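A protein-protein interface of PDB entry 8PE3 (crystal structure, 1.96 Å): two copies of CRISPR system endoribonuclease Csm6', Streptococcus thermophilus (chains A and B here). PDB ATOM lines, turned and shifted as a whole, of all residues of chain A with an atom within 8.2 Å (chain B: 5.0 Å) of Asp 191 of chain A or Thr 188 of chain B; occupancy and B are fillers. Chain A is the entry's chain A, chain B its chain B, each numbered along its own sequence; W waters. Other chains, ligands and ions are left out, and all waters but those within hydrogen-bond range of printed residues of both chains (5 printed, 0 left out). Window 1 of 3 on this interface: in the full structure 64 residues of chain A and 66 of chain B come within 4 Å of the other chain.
The guanidinium group (NH2) of Arg 190 of chain B sits at hydrogen-bond distance from the backbone carbonyl oxygen (O) of Leu 125 of chain A, at 3.3 Å. The side-chain amino group of Lys 187 of chain B sits at hydrogen-bond distance from the side-chain hydroxyl of Thr 188 of chain A. The side-chain hydroxyl (OG1) of Thr 188 of chain A is in hydrogen-bond range of the side-chain carboxylate (OD2) of Asp 191 of chain B. OG1 of Thr 188 of chain B lies within hydrogen-bond range of OD2 of Asp 191 of chain A, at 2.6 Å.
The backbone carbonyl oxygen (O) of Leu 184 of chain A sits at hydrogen-bond distance from the side-chain hydroxyl (OG1) of Thr 188 of chain A (3.2 Å). The side-chain amino group (NZ) of Lys 187 of chain A is in salt-bridge range of the side-chain carboxylate (OD1) of Asp 191 of chain A, at 3.4 Å. The backbone carbonyl oxygen of Phe 192 of chain A lies within hydrogen-bond range of the backbone NH of Asp 197 of chain A. OG1 of Thr 188 of chain B lies within hydrogen-bond range of O of Leu 184 of chain B (3.0 Å). NZ of Lys 187 of chain B lies within salt-bridge range of OD2 of Asp 191 of chain B (2.9 Å).
Leu 184 of chain B touches Leu 125 of chain A. Lys 187 of chain B touches Leu 125 of chain A (CD to O, 3.3 Å). Thr 188 of chain B touches Lys 187 of chain A. Asp 191 of chain A touches Phe 192 of chain B. Asp 191 of chain B touches Phe 192 of chain A. Phe 192 of chain A touches Phe 192 of chain B. Lys 195 of chain A touches Phe 192 of chain B (CG to CZ, 3.5 Å).
Of chain B, only Thr 188 (2.6 Å) and Phe 192 (3.6 Å) come within 4 Å of Asp 191 of chain A. Thr 188 of chain B touches just these residues of chain A: Lys 187 and Asp 191. Of the printed residues of chain B, Lys 187 of chain A touches Thr 188 (3.6 Å). Printed residues of chain A within 4 Å of Leu 184 of chain B: Leu 125 (3.7 Å). Printed residues of chain A within 4 Å of Arg 190 of chain B: Leu 125 (3.3 Å). Arg 190 of chain A touches none of the printed residues of chain B. Asn 382 of chain A touches none of the printed residues of chain B. The nearest printed residue of chain B that does not touch Asp 191 of chain A is Asp 191 of chain B (5.0 Å). The nearest printed residue of chain A that does not touch Leu 184 of chain B is Lys 187 of chain A (4.5 Å).
Of the 20 printed residues of chain A, 6 touch a printed residue of chain B. Hydrophobic or aromatic side chains of chain A within 4 Å of the printed part of chain B: Leu 125 and Phe 192. Along chain B the printed residues that touch a printed residue of chain A span positions 184 to 192. Among the printed residues, no Asp or Glu carboxylate lies within 4 Å of a Lys or Arg side-chain nitrogen of the other chain.
Lys 187 of chain A touches Thr 188 of chain B, and with the chains exchanged Thr 188 of chain A touches Lys 187 of chain B. Thr 188 of chain A touches Asp 191 of chain B, and with the chains exchanged Asp 191 of chain A touches Thr 188 of chain B. Asp 191 of chain A touches Phe 192 of chain B, and with the chains exchanged Phe 192 of chain A touches Asp 191 of chain B. Phe 192 of chain A touches its own counterpart, Phe 192 of chain B.
Water W4 bridges the side-chain hydroxyl (OG1) of Thr 188 of chain A (2.6 Å) and the side-chain amino group (NZ) of Lys 187 of chain B (3.2 Å). Water W2 lies within hydrogen-bond range of the side-chain hydroxyl of Thr 188 of chain B and the side-chain amino group of Lys 187 of chain A. Water W3 lies within hydrogen-bond range of OD2 of Asp 191 of chain A, OD2 of Asp 191 of chain B, OG1 of Thr 188 of chain A and OG1 of Thr 188 of chain B. Water W5 lies within hydrogen-bond range of O of Leu 184 of chain A, NZ of Lys 187 of chain B and OG1 of Thr 188 of chain A. Water W1 lies within hydrogen-bond range of NZ of Lys 187 of chain A (3.0 Å), O of Leu 184 of chain B (3.1 Å) and OG1 of Thr 188 of chain B (3.1 Å).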
ATOM      1  N   LEU A 125     -12.819 -37.970 -10.895  1.00  0.00           N
ATOM      2  CA  LEU A 125     -14.110 -37.305 -11.022  1.00  0.00           C
ATOM      3  C   LEU A 125     -15.257 -38.294 -10.830  1.00  0.00           C
ATOM      4  O   LEU A 125     -16.247 -37.980 -10.161  1.00  0.00           O
ATOM      5  CB  LEU A 125     -14.199 -36.607 -12.377  1.00  0.00           C
ATOM      6  CG  LEU A 125     -15.465 -35.798 -12.636  1.00  0.00           C
ATOM      7  CD1 LEU A 125     -15.593 -34.714 -11.600  1.00  0.00           C
ATOM      8  CD2 LEU A 125     -15.418 -35.194 -14.029  1.00  0.00           C
ATOM      9  N   LEU A 184     -11.184 -31.637  -5.649  1.00  0.00           N
ATOM     10  CA  LEU A 184     -12.519 -32.180  -5.873  1.00  0.00           C
ATOM     11  C   LEU A 184     -13.349 -32.134  -4.599  1.00  0.00           C
ATOM     12  O   LEU A 184     -14.544 -31.811  -4.636  1.00  0.00           O
ATOM     13  CB  LEU A 184     -12.421 -33.610  -6.408  1.00  0.00           C
ATOM     14  CG  LEU A 184     -11.990 -33.744  -7.869  1.00  0.00           C
ATOM     15  CD1 LEU A 184     -11.831 -35.204  -8.239  1.00  0.00           C
ATOM     16  CD2 LEU A 184     -13.008 -33.067  -8.780  1.00  0.00           C
ATOM     17  N   LEU A 185     -12.733 -32.443  -3.459  1.00  0.00           N
ATOM     18  CA  LEU A 185     -13.452 -32.365  -2.195  1.00  0.00           C
ATOM     19  C   LEU A 185     -13.831 -30.924  -1.878  1.00  0.00           C
ATOM     20  O   LEU A 185     -14.961 -30.641  -1.457  1.00  0.00           O
ATOM     21  CB  LEU A 185     -12.600 -32.964  -1.079  1.00  0.00           C
ATOM     22  CG  LEU A 185     -12.563 -34.495  -1.035  1.00  0.00           C
ATOM     23  CD1 LEU A 185     -11.457 -34.963  -0.111  1.00  0.00           C
ATOM     24  CD2 LEU A 185     -13.898 -35.050  -0.580  1.00  0.00           C
ATOM     25  N   LYS A 186     -12.895 -29.993  -2.079  1.00  0.00           N
ATOM     26  CA  LYS A 186     -13.199 -28.585  -1.848  1.00  0.00           C
ATOM     27  C   LYS A 186     -14.327 -28.118  -2.752  1.00  0.00           C
ATOM     28  O   LYS A 186     -15.180 -27.324  -2.338  1.00  0.00           O
ATOM     29  CB  LYS A 186     -11.967 -27.723  -2.094  1.00  0.00           C
ATOM     30  CG  LYS A 186     -10.881 -27.813  -1.064  1.00  0.00           C
ATOM     31  CD  LYS A 186     -10.091 -26.528  -1.167  1.00  0.00           C
ATOM     32  CE  LYS A 186      -8.604 -26.724  -1.049  1.00  0.00           C
ATOM     33  NZ  LYS A 186      -7.936 -25.529  -1.655  1.00  0.00           N
ATOM     34  N   LYS A 187     -14.327 -28.579  -4.002  1.00  0.00           N
ATOM     35  CA  LYS A 187     -15.419 -28.249  -4.907  1.00  0.00           C
ATOM     36  C   LYS A 187     -16.751 -28.711  -4.335  1.00  0.00           C
ATOM     37  O   LYS A 187     -17.742 -27.972  -4.363  1.00  0.00           O
ATOM     38  CB  LYS A 187     -15.155 -28.881  -6.272  1.00  0.00           C
ATOM     39  CG  LYS A 187     -16.355 -28.951  -7.184  1.00  0.00           C
ATOM     40  CD  LYS A 187     -16.532 -27.659  -7.920  1.00  0.00           C
ATOM     41  CE  LYS A 187     -17.143 -27.902  -9.290  1.00  0.00           C
ATOM     42  NZ  LYS A 187     -18.635 -27.777  -9.230  1.00  0.00           N
ATOM     43  N   THR A 188     -16.788 -29.916  -3.773  1.00  0.00           N
ATOM     44  CA  THR A 188     -18.019 -30.385  -3.150  1.00  0.00           C
ATOM     45  C   THR A 188     -18.389 -29.525  -1.948  1.00  0.00           C
ATOM     46  O   THR A 188     -19.560 -29.171  -1.774  1.00  0.00           O
ATOM     47  CB  THR A 188     -17.879 -31.844  -2.736  1.00  0.00           C
ATOM     48  OG1 THR A 188     -17.568 -32.637  -3.885  1.00  0.00           O
ATOM     49  CG2 THR A 188     -19.170 -32.331  -2.144  1.00  0.00           C
ATOM     50  N   ALA A 189     -17.414 -29.182  -1.102  1.00  0.00           N
ATOM     51  CA  ALA A 189     -17.720 -28.320   0.035  1.00  0.00           C
ATOM     52  C   ALA A 189     -18.319 -26.999  -0.434  1.00  0.00           C
ATOM     53  O   ALA A 189     -19.299 -26.510   0.146  1.00  0.00           O
ATOM     54  CB  ALA A 189     -16.462 -28.080   0.870  1.00  0.00           C
ATOM     55  N   ARG A 190     -17.764 -26.429  -1.507  1.00  0.00           N
ATOM     56  CA  ARG A 190     -18.296 -25.185  -2.050  1.00  0.00           C
ATOM     57  C   ARG A 190     -19.706 -25.378  -2.592  1.00  0.00           C
ATOM     58  O   ARG A 190     -20.576 -24.522  -2.396  1.00  0.00           O
ATOM     59  CB  ARG A 190     -17.372 -24.657  -3.146  1.00  0.00           C
ATOM     60  CG  ARG A 190     -16.018 -24.187  -2.638  1.00  0.00           C
ATOM     61  CD  ARG A 190     -15.335 -23.267  -3.635  1.00  0.00           C
ATOM     62  NE  ARG A 190     -15.235 -23.878  -4.957  1.00  0.00           N
ATOM     63  CZ  ARG A 190     -14.204 -24.605  -5.369  1.00  0.00           C
ATOM     64  NH1 ARG A 190     -13.158 -24.829  -4.587  1.00  0.00           N
ATOM     65  NH2 ARG A 190     -14.220 -25.119  -6.598  1.00  0.00           N
ATOM     66  N   ASP A 191     -19.950 -26.490  -3.293  1.00  0.00           N
ATOM     67  CA  ASP A 191     -21.296 -26.762  -3.794  1.00  0.00           C
ATOM     68  C   ASP A 191     -22.290 -26.829  -2.644  1.00  0.00           C
ATOM     69  O   ASP A 191     -23.393 -26.270  -2.717  1.00  0.00           O
ATOM     70  CB  ASP A 191     -21.316 -28.072  -4.591  1.00  0.00           C
ATOM     71  CG  ASP A 191     -20.582 -27.973  -5.909  1.00  0.00           C
ATOM     72  OD1 ASP A 191     -20.201 -26.840  -6.311  1.00  0.00           O
ATOM     73  OD2 ASP A 191     -20.381 -29.041  -6.542  1.00  0.00           O
ATOM     74  N   PHE A 192     -21.907 -27.509  -1.563  1.00  0.00           N
ATOM     75  CA  PHE A 192     -22.784 -27.624  -0.408  1.00  0.00           C
ATOM     76  C   PHE A 192     -23.060 -26.268   0.210  1.00  0.00           C
ATOM     77  O   PHE A 192     -24.193 -25.983   0.617  1.00  0.00           O
ATOM     78  CB  PHE A 192     -22.158 -28.552   0.628  1.00  0.00           C
ATOM     79  CG  PHE A 192     -22.299 -30.003   0.293  1.00  0.00           C
ATOM     80  CD1 PHE A 192     -23.402 -30.458  -0.406  1.00  0.00           C
ATOM     81  CD2 PHE A 192     -21.336 -30.911   0.675  1.00  0.00           C
ATOM     82  CE1 PHE A 192     -23.539 -31.793  -0.723  1.00  0.00           C
ATOM     83  CE2 PHE A 192     -21.473 -32.247   0.362  1.00  0.00           C
ATOM     84  CZ  PHE A 192     -22.575 -32.688  -0.340  1.00  0.00           C
ATOM     85  N   ILE A 193     -22.037 -25.418   0.297  1.00  0.00           N
ATOM     86  CA  ILE A 193     -22.204 -24.124   0.955  1.00  0.00           C
ATOM     87  C   ILE A 193     -23.144 -23.238   0.147  1.00  0.00           C
ATOM     88  O   ILE A 193     -24.057 -22.607   0.694  1.00  0.00           O
ATOM     89  CB  ILE A 193     -20.834 -23.458   1.171  1.00  0.00           C
ATOM     90  CG1 ILE A 193     -20.086 -24.142   2.314  1.00  0.00           C
ATOM     91  CG2 ILE A 193     -20.995 -21.980   1.439  1.00  0.00           C
ATOM     92  CD1 ILE A 193     -18.594 -23.971   2.209  1.00  0.00           C
ATOM     93  N   GLU A 194     -22.946 -23.192  -1.170  1.00  0.00           N
ATOM     94  CA  GLU A 194     -23.824 -22.403  -2.026  1.00  0.00           C
ATOM     95  C   GLU A 194     -25.291 -22.741  -1.800  1.00  0.00           C
ATOM     96  O   GLU A 194     -26.158 -21.870  -1.929  1.00  0.00           O
ATOM     97  CB  GLU A 194     -23.466 -22.627  -3.496  1.00  0.00           C
ATOM     98  CG  GLU A 194     -22.511 -21.604  -4.085  1.00  0.00           C
ATOM     99  CD  GLU A 194     -21.917 -22.065  -5.408  1.00  0.00           C
ATOM    100  OE1 GLU A 194     -22.545 -21.799  -6.459  1.00  0.00           O
ATOM    101  OE2 GLU A 194     -20.828 -22.692  -5.398  1.00  0.00           O
ATOM    102  N   LYS A 195     -25.590 -23.988  -1.445  1.00  0.00           N
ATOM    103  CA  LYS A 195     -26.960 -24.439  -1.265  1.00  0.00           C
ATOM    104  C   LYS A 195     -27.359 -24.543   0.199  1.00  0.00           C
ATOM    105  O   LYS A 195     -28.430 -25.079   0.503  1.00  0.00           O
ATOM    106  CB  LYS A 195     -27.153 -25.782  -1.959  1.00  0.00           C
ATOM    107  CG  LYS A 195     -26.991 -25.688  -3.457  1.00  0.00           C
ATOM    108  CD  LYS A 195     -28.315 -25.378  -4.099  1.00  0.00           C
ATOM    109  CE  LYS A 195     -28.139 -24.876  -5.517  1.00  0.00           C
ATOM    110  NZ  LYS A 195     -28.692 -25.865  -6.499  1.00  0.00           N
ATOM    111  N   PHE A 196     -26.518 -24.053   1.106  1.00  0.00           N
ATOM    112  CA  PHE A 196     -26.792 -23.889   2.527  1.00  0.00           C
ATOM    113  C   PHE A 196     -26.752 -25.196   3.304  1.00  0.00           C
ATOM    114  O   PHE A 196     -27.148 -25.198   4.475  1.00  0.00           O
ATOM    115  CB  PHE A 196     -28.134 -23.190   2.765  1.00  0.00           C
ATOM    116  CG  PHE A 196     -28.261 -21.899   2.023  1.00  0.00           C
ATOM    117  CD1 PHE A 196     -27.532 -20.790   2.418  1.00  0.00           C
ATOM    118  CD2 PHE A 196     -29.067 -21.803   0.898  1.00  0.00           C
ATOM    119  CE1 PHE A 196     -27.629 -19.592   1.724  1.00  0.00           C
ATOM    120  CE2 PHE A 196     -29.162 -20.613   0.192  1.00  0.00           C
ATOM    121  CZ  PHE A 196     -28.443 -19.505   0.607  1.00  0.00           C
ATOM    122  N   ASP A 197     -26.290 -26.301   2.717  1.00  0.00           N
ATOM    123  CA  ASP A 197     -26.029 -27.503   3.511  1.00  0.00           C
ATOM    124  C   ASP A 197     -24.711 -27.323   4.238  1.00  0.00           C
ATOM    125  O   ASP A 197     -23.652 -27.789   3.814  1.00  0.00           O
ATOM    126  CB  ASP A 197     -26.018 -28.772   2.672  1.00  0.00           C
ATOM    127  CG  ASP A 197     -26.344 -30.012   3.511  1.00  0.00           C
ATOM    128  OD1 ASP A 197     -26.867 -31.000   2.954  1.00  0.00           O
ATOM    129  OD2 ASP A 197     -26.074 -29.995   4.741  1.00  0.00           O
ATOM    130  N   ALA A 200     -23.303 -30.794   5.786  1.00  0.00           N
ATOM    131  CA  ALA A 200     -22.600 -31.597   4.791  1.00  0.00           C
ATOM    132  C   ALA A 200     -21.271 -30.957   4.410  1.00  0.00           C
ATOM    133  O   ALA A 200     -20.266 -31.655   4.230  1.00  0.00           O
ATOM    134  CB  ALA A 200     -23.481 -31.792   3.561  1.00  0.00           C
ATOM    135  N   ALA A 201     -21.246 -29.629   4.282  1.00  0.00           N
ATOM    136  CA  ALA A 201     -19.987 -28.942   4.011  1.00  0.00           C
ATOM    137  C   ALA A 201     -18.982 -29.184   5.127  1.00  0.00           C
ATOM    138  O   ALA A 201     -17.797 -29.426   4.866  1.00  0.00           O
ATOM    139  CB  ALA A 201     -20.234 -27.447   3.836  1.00  0.00           C
ATOM    140  N   ASN A 382     -21.549 -16.856   2.725  1.00  0.00           N
ATOM    141  CA  ASN A 382     -21.133 -17.802   1.696  1.00  0.00           C
ATOM    142  C   ASN A 382     -20.064 -17.204   0.799  1.00  0.00           C
ATOM    143  O   ASN A 382     -19.082 -17.876   0.461  1.00  0.00           O
ATOM    144  CB  ASN A 382     -22.336 -18.237   0.863  1.00  0.00           C
ATOM    145  CG  ASN A 382     -23.217 -19.221   1.587  1.00  0.00           C
ATOM    146  OD1 ASN A 382     -22.963 -19.585   2.741  1.00  0.00           O
ATOM    147  ND2 ASN A 382     -24.278 -19.653   0.919  1.00  0.00           N
ATOM    148  N   LEU A 386     -16.580 -19.034   0.333  1.00  0.00           N
ATOM    149  CA  LEU A 386     -16.231 -19.651  -0.938  1.00  0.00           C
ATOM    150  C   LEU A 386     -14.861 -19.188  -1.412  1.00  0.00           C
ATOM    151  O   LEU A 386     -14.063 -20.001  -1.892  1.00  0.00           O
ATOM    152  CB  LEU A 386     -17.297 -19.354  -1.992  1.00  0.00           C
ATOM    153  CG  LEU A 386     -18.660 -20.030  -1.803  1.00  0.00           C
ATOM    154  CD1 LEU A 386     -19.552 -19.749  -2.990  1.00  0.00           C
ATOM    155  CD2 LEU A 386     -18.506 -21.521  -1.593  1.00  0.00           C
ATOM    156  N   LEU A 389     -12.013 -20.972   0.070  1.00  0.00           N
ATOM    157  CA  LEU A 389     -11.873 -22.376  -0.318  1.00  0.00           C
ATOM    158  C   LEU A 389     -11.416 -22.529  -1.766  1.00  0.00           C
ATOM    159  O   LEU A 389     -11.848 -23.445  -2.472  1.00  0.00           O
ATOM    160  CB  LEU A 389     -13.175 -23.143  -0.094  1.00  0.00           C
ATOM    161  CG  LEU A 389     -13.572 -23.406   1.362  1.00  0.00           C
ATOM    162  CD1 LEU A 389     -15.057 -23.697   1.482  1.00  0.00           C
ATOM    163  CD2 LEU A 389     -12.768 -24.561   1.937  1.00  0.00           C
ATOM    164  N   LEU B 184     -19.151 -32.231 -14.464  1.00  0.00           N
ATOM    165  CA  LEU B 184     -19.001 -31.568 -13.173  1.00  0.00           C
ATOM    166  C   LEU B 184     -20.358 -31.283 -12.544  1.00  0.00           C
ATOM    167  O   LEU B 184     -20.509 -31.349 -11.315  1.00  0.00           O
ATOM    168  CB  LEU B 184     -18.198 -30.274 -13.339  1.00  0.00           C
ATOM    169  CG  LEU B 184     -16.727 -30.413 -13.751  1.00  0.00           C
ATOM    170  CD1 LEU B 184     -16.088 -29.030 -13.971  1.00  0.00           C
ATOM    171  CD2 LEU B 184     -15.945 -31.206 -12.706  1.00  0.00           C
ATOM    172  N   LEU B 185     -21.359 -30.950 -13.365  1.00  0.00           N
ATOM    173  CA  LEU B 185     -22.702 -30.758 -12.827  1.00  0.00           C
ATOM    174  C   LEU B 185     -23.276 -32.074 -12.328  1.00  0.00           C
ATOM    175  O   LEU B 185     -23.895 -32.123 -11.262  1.00  0.00           O
ATOM    176  CB  LEU B 185     -23.621 -30.151 -13.885  1.00  0.00           C
ATOM    177  CG  LEU B 185     -23.411 -28.670 -14.204  1.00  0.00           C
ATOM    178  CD1 LEU B 185     -24.296 -28.269 -15.358  1.00  0.00           C
ATOM    179  CD2 LEU B 185     -23.720 -27.829 -12.992  1.00  0.00           C
ATOM    180  N   LYS B 186     -23.091 -33.147 -13.094  1.00  0.00           N
ATOM    181  CA  LYS B 186     -23.546 -34.453 -12.647  1.00  0.00           C
ATOM    182  C   LYS B 186     -22.884 -34.827 -11.327  1.00  0.00           C
ATOM    183  O   LYS B 186     -23.548 -35.314 -10.406  1.00  0.00           O
ATOM    184  CB  LYS B 186     -23.246 -35.489 -13.729  1.00  0.00           C
ATOM    185  CG  LYS B 186     -24.336 -35.647 -14.795  1.00  0.00           C
ATOM    186  CD  LYS B 186     -23.719 -36.005 -16.152  1.00  0.00           C
ATOM    187  CE  LYS B 186     -24.440 -37.134 -16.855  1.00  0.00           C
ATOM    188  NZ  LYS B 186     -24.055 -38.454 -16.272  1.00  0.00           N
ATOM    189  N   LYS B 187     -21.575 -34.581 -11.209  1.00  0.00           N
ATOM    190  CA  LYS B 187     -20.879 -34.860  -9.954  1.00  0.00           C
ATOM    191  C   LYS B 187     -21.498 -34.083  -8.796  1.00  0.00           C
ATOM    192  O   LYS B 187     -21.698 -34.628  -7.704  1.00  0.00           O
ATOM    193  CB  LYS B 187     -19.393 -34.535 -10.101  1.00  0.00           C
ATOM    194  CG  LYS B 187     -18.639 -34.456  -8.788  1.00  0.00           C
ATOM    195  CD  LYS B 187     -17.936 -35.760  -8.486  1.00  0.00           C
ATOM    196  CE  LYS B 187     -16.812 -35.562  -7.480  1.00  0.00           C
ATOM    197  NZ  LYS B 187     -17.367 -35.183  -6.149  1.00  0.00           N
ATOM    198  N   THR B 188     -21.835 -32.813  -9.017  1.00  0.00           N
ATOM    199  CA  THR B 188     -22.499 -32.045  -7.970  1.00  0.00           C
ATOM    200  C   THR B 188     -23.848 -32.658  -7.604  1.00  0.00           C
ATOM    201  O   THR B 188     -24.191 -32.774  -6.422  1.00  0.00           O
ATOM    202  CB  THR B 188     -22.684 -30.602  -8.418  1.00  0.00           C
ATOM    203  OG1 THR B 188     -21.410 -30.032  -8.743  1.00  0.00           O
ATOM    204  CG2 THR B 188     -23.335 -29.810  -7.313  1.00  0.00           C
ATOM    205  N   ALA B 189     -24.637 -33.042  -8.613  1.00  0.00           N
ATOM    206  CA  ALA B 189     -25.924 -33.679  -8.351  1.00  0.00           C
ATOM    207  C   ALA B 189     -25.746 -34.977  -7.578  1.00  0.00           C
ATOM    208  O   ALA B 189     -26.500 -35.260  -6.640  1.00  0.00           O
ATOM    209  CB  ALA B 189     -26.658 -33.940  -9.665  1.00  0.00           C
ATOM    210  N   ARG B 190     -24.757 -35.781  -7.957  1.00  0.00           N
ATOM    211  CA  ARG B 190     -24.454 -36.986  -7.195  1.00  0.00           C
ATOM    212  C   ARG B 190     -24.119 -36.644  -5.750  1.00  0.00           C
ATOM    213  O   ARG B 190     -24.626 -37.272  -4.812  1.00  0.00           O
ATOM    214  CB  ARG B 190     -23.303 -37.745  -7.857  1.00  0.00           C
ATOM    215  CG  ARG B 190     -23.669 -38.412  -9.165  1.00  0.00           C
ATOM    216  CD  ARG B 190     -22.716 -39.560  -9.482  1.00  0.00           C
ATOM    217  NE  ARG B 190     -21.327 -39.116  -9.583  1.00  0.00           N
ATOM    218  CZ  ARG B 190     -20.806 -38.541 -10.657  1.00  0.00           C
ATOM    219  NH1 ARG B 190     -21.536 -38.314 -11.741  1.00  0.00           N
ATOM    220  NH2 ARG B 190     -19.524 -38.181 -10.646  1.00  0.00           N
ATOM    221  N   ASP B 191     -23.277 -35.626  -5.553  1.00  0.00           N
ATOM    222  CA  ASP B 191     -22.855 -35.264  -4.203  1.00  0.00           C
ATOM    223  C   ASP B 191     -24.047 -34.847  -3.355  1.00  0.00           C
ATOM    224  O   ASP B 191     -24.119 -35.169  -2.160  1.00  0.00           O
ATOM    225  CB  ASP B 191     -21.830 -34.134  -4.265  1.00  0.00           C
ATOM    226  CG  ASP B 191     -20.469 -34.613  -4.723  1.00  0.00           C
ATOM    227  OD1 ASP B 191     -20.187 -35.830  -4.597  1.00  0.00           O
ATOM    228  OD2 ASP B 191     -19.665 -33.767  -5.178  1.00  0.00           O
ATOM    229  N   PHE B 192     -25.005 -34.138  -3.964  1.00  0.00           N
ATOM    230  CA  PHE B 192     -26.208 -33.735  -3.244  1.00  0.00           C
ATOM    231  C   PHE B 192     -27.050 -34.943  -2.868  1.00  0.00           C
ATOM    232  O   PHE B 192     -27.562 -35.034  -1.747  1.00  0.00           O
ATOM    233  CB  PHE B 192     -27.030 -32.774  -4.100  1.00  0.00           C
ATOM    234  CG  PHE B 192     -26.487 -31.370  -4.144  1.00  0.00           C
ATOM    235  CD1 PHE B 192     -25.844 -30.818  -3.046  1.00  0.00           C
ATOM    236  CD2 PHE B 192     -26.646 -30.590  -5.280  1.00  0.00           C
ATOM    237  CE1 PHE B 192     -25.355 -29.520  -3.089  1.00  0.00           C
ATOM    238  CE2 PHE B 192     -26.168 -29.295  -5.327  1.00  0.00           C
ATOM    239  CZ  PHE B 192     -25.517 -28.758  -4.231  1.00  0.00           C
ATOM    240  N   ILE B 204     -30.066 -28.935 -10.125  1.00  0.00           N
ATOM    241  CA  ILE B 204     -29.002 -29.230 -11.083  1.00  0.00           C
ATOM    242  C   ILE B 204     -29.556 -30.005 -12.274  1.00  0.00           C
ATOM    243  O   ILE B 204     -29.292 -29.667 -13.435  1.00  0.00           O
ATOM    244  CB  ILE B 204     -27.863 -30.010 -10.404  1.00  0.00           C
ATOM    245  CG1 ILE B 204     -27.296 -29.252  -9.199  1.00  0.00           C
ATOM    246  CG2 ILE B 204     -26.801 -30.341 -11.414  1.00  0.00           C
ATOM    247  CD1 ILE B 204     -26.084 -28.434  -9.508  1.00  0.00           C
HETATM  248  O   HOH W   1     -18.405 -30.742  -9.185  1.00  0.00           O
HETATM  249  O   HOH W   2     -21.533 -27.944 -10.462  1.00  0.00           O
HETATM  250  O   HOH W   3     -18.951 -31.426  -6.749  1.00  0.00           O
HETATM  251  O   HOH W   4     -16.238 -34.802  -3.168  1.00  0.00           O
HETATM  252  O   HOH W   5     -16.366 -32.430  -6.818  1.00  0.00           O
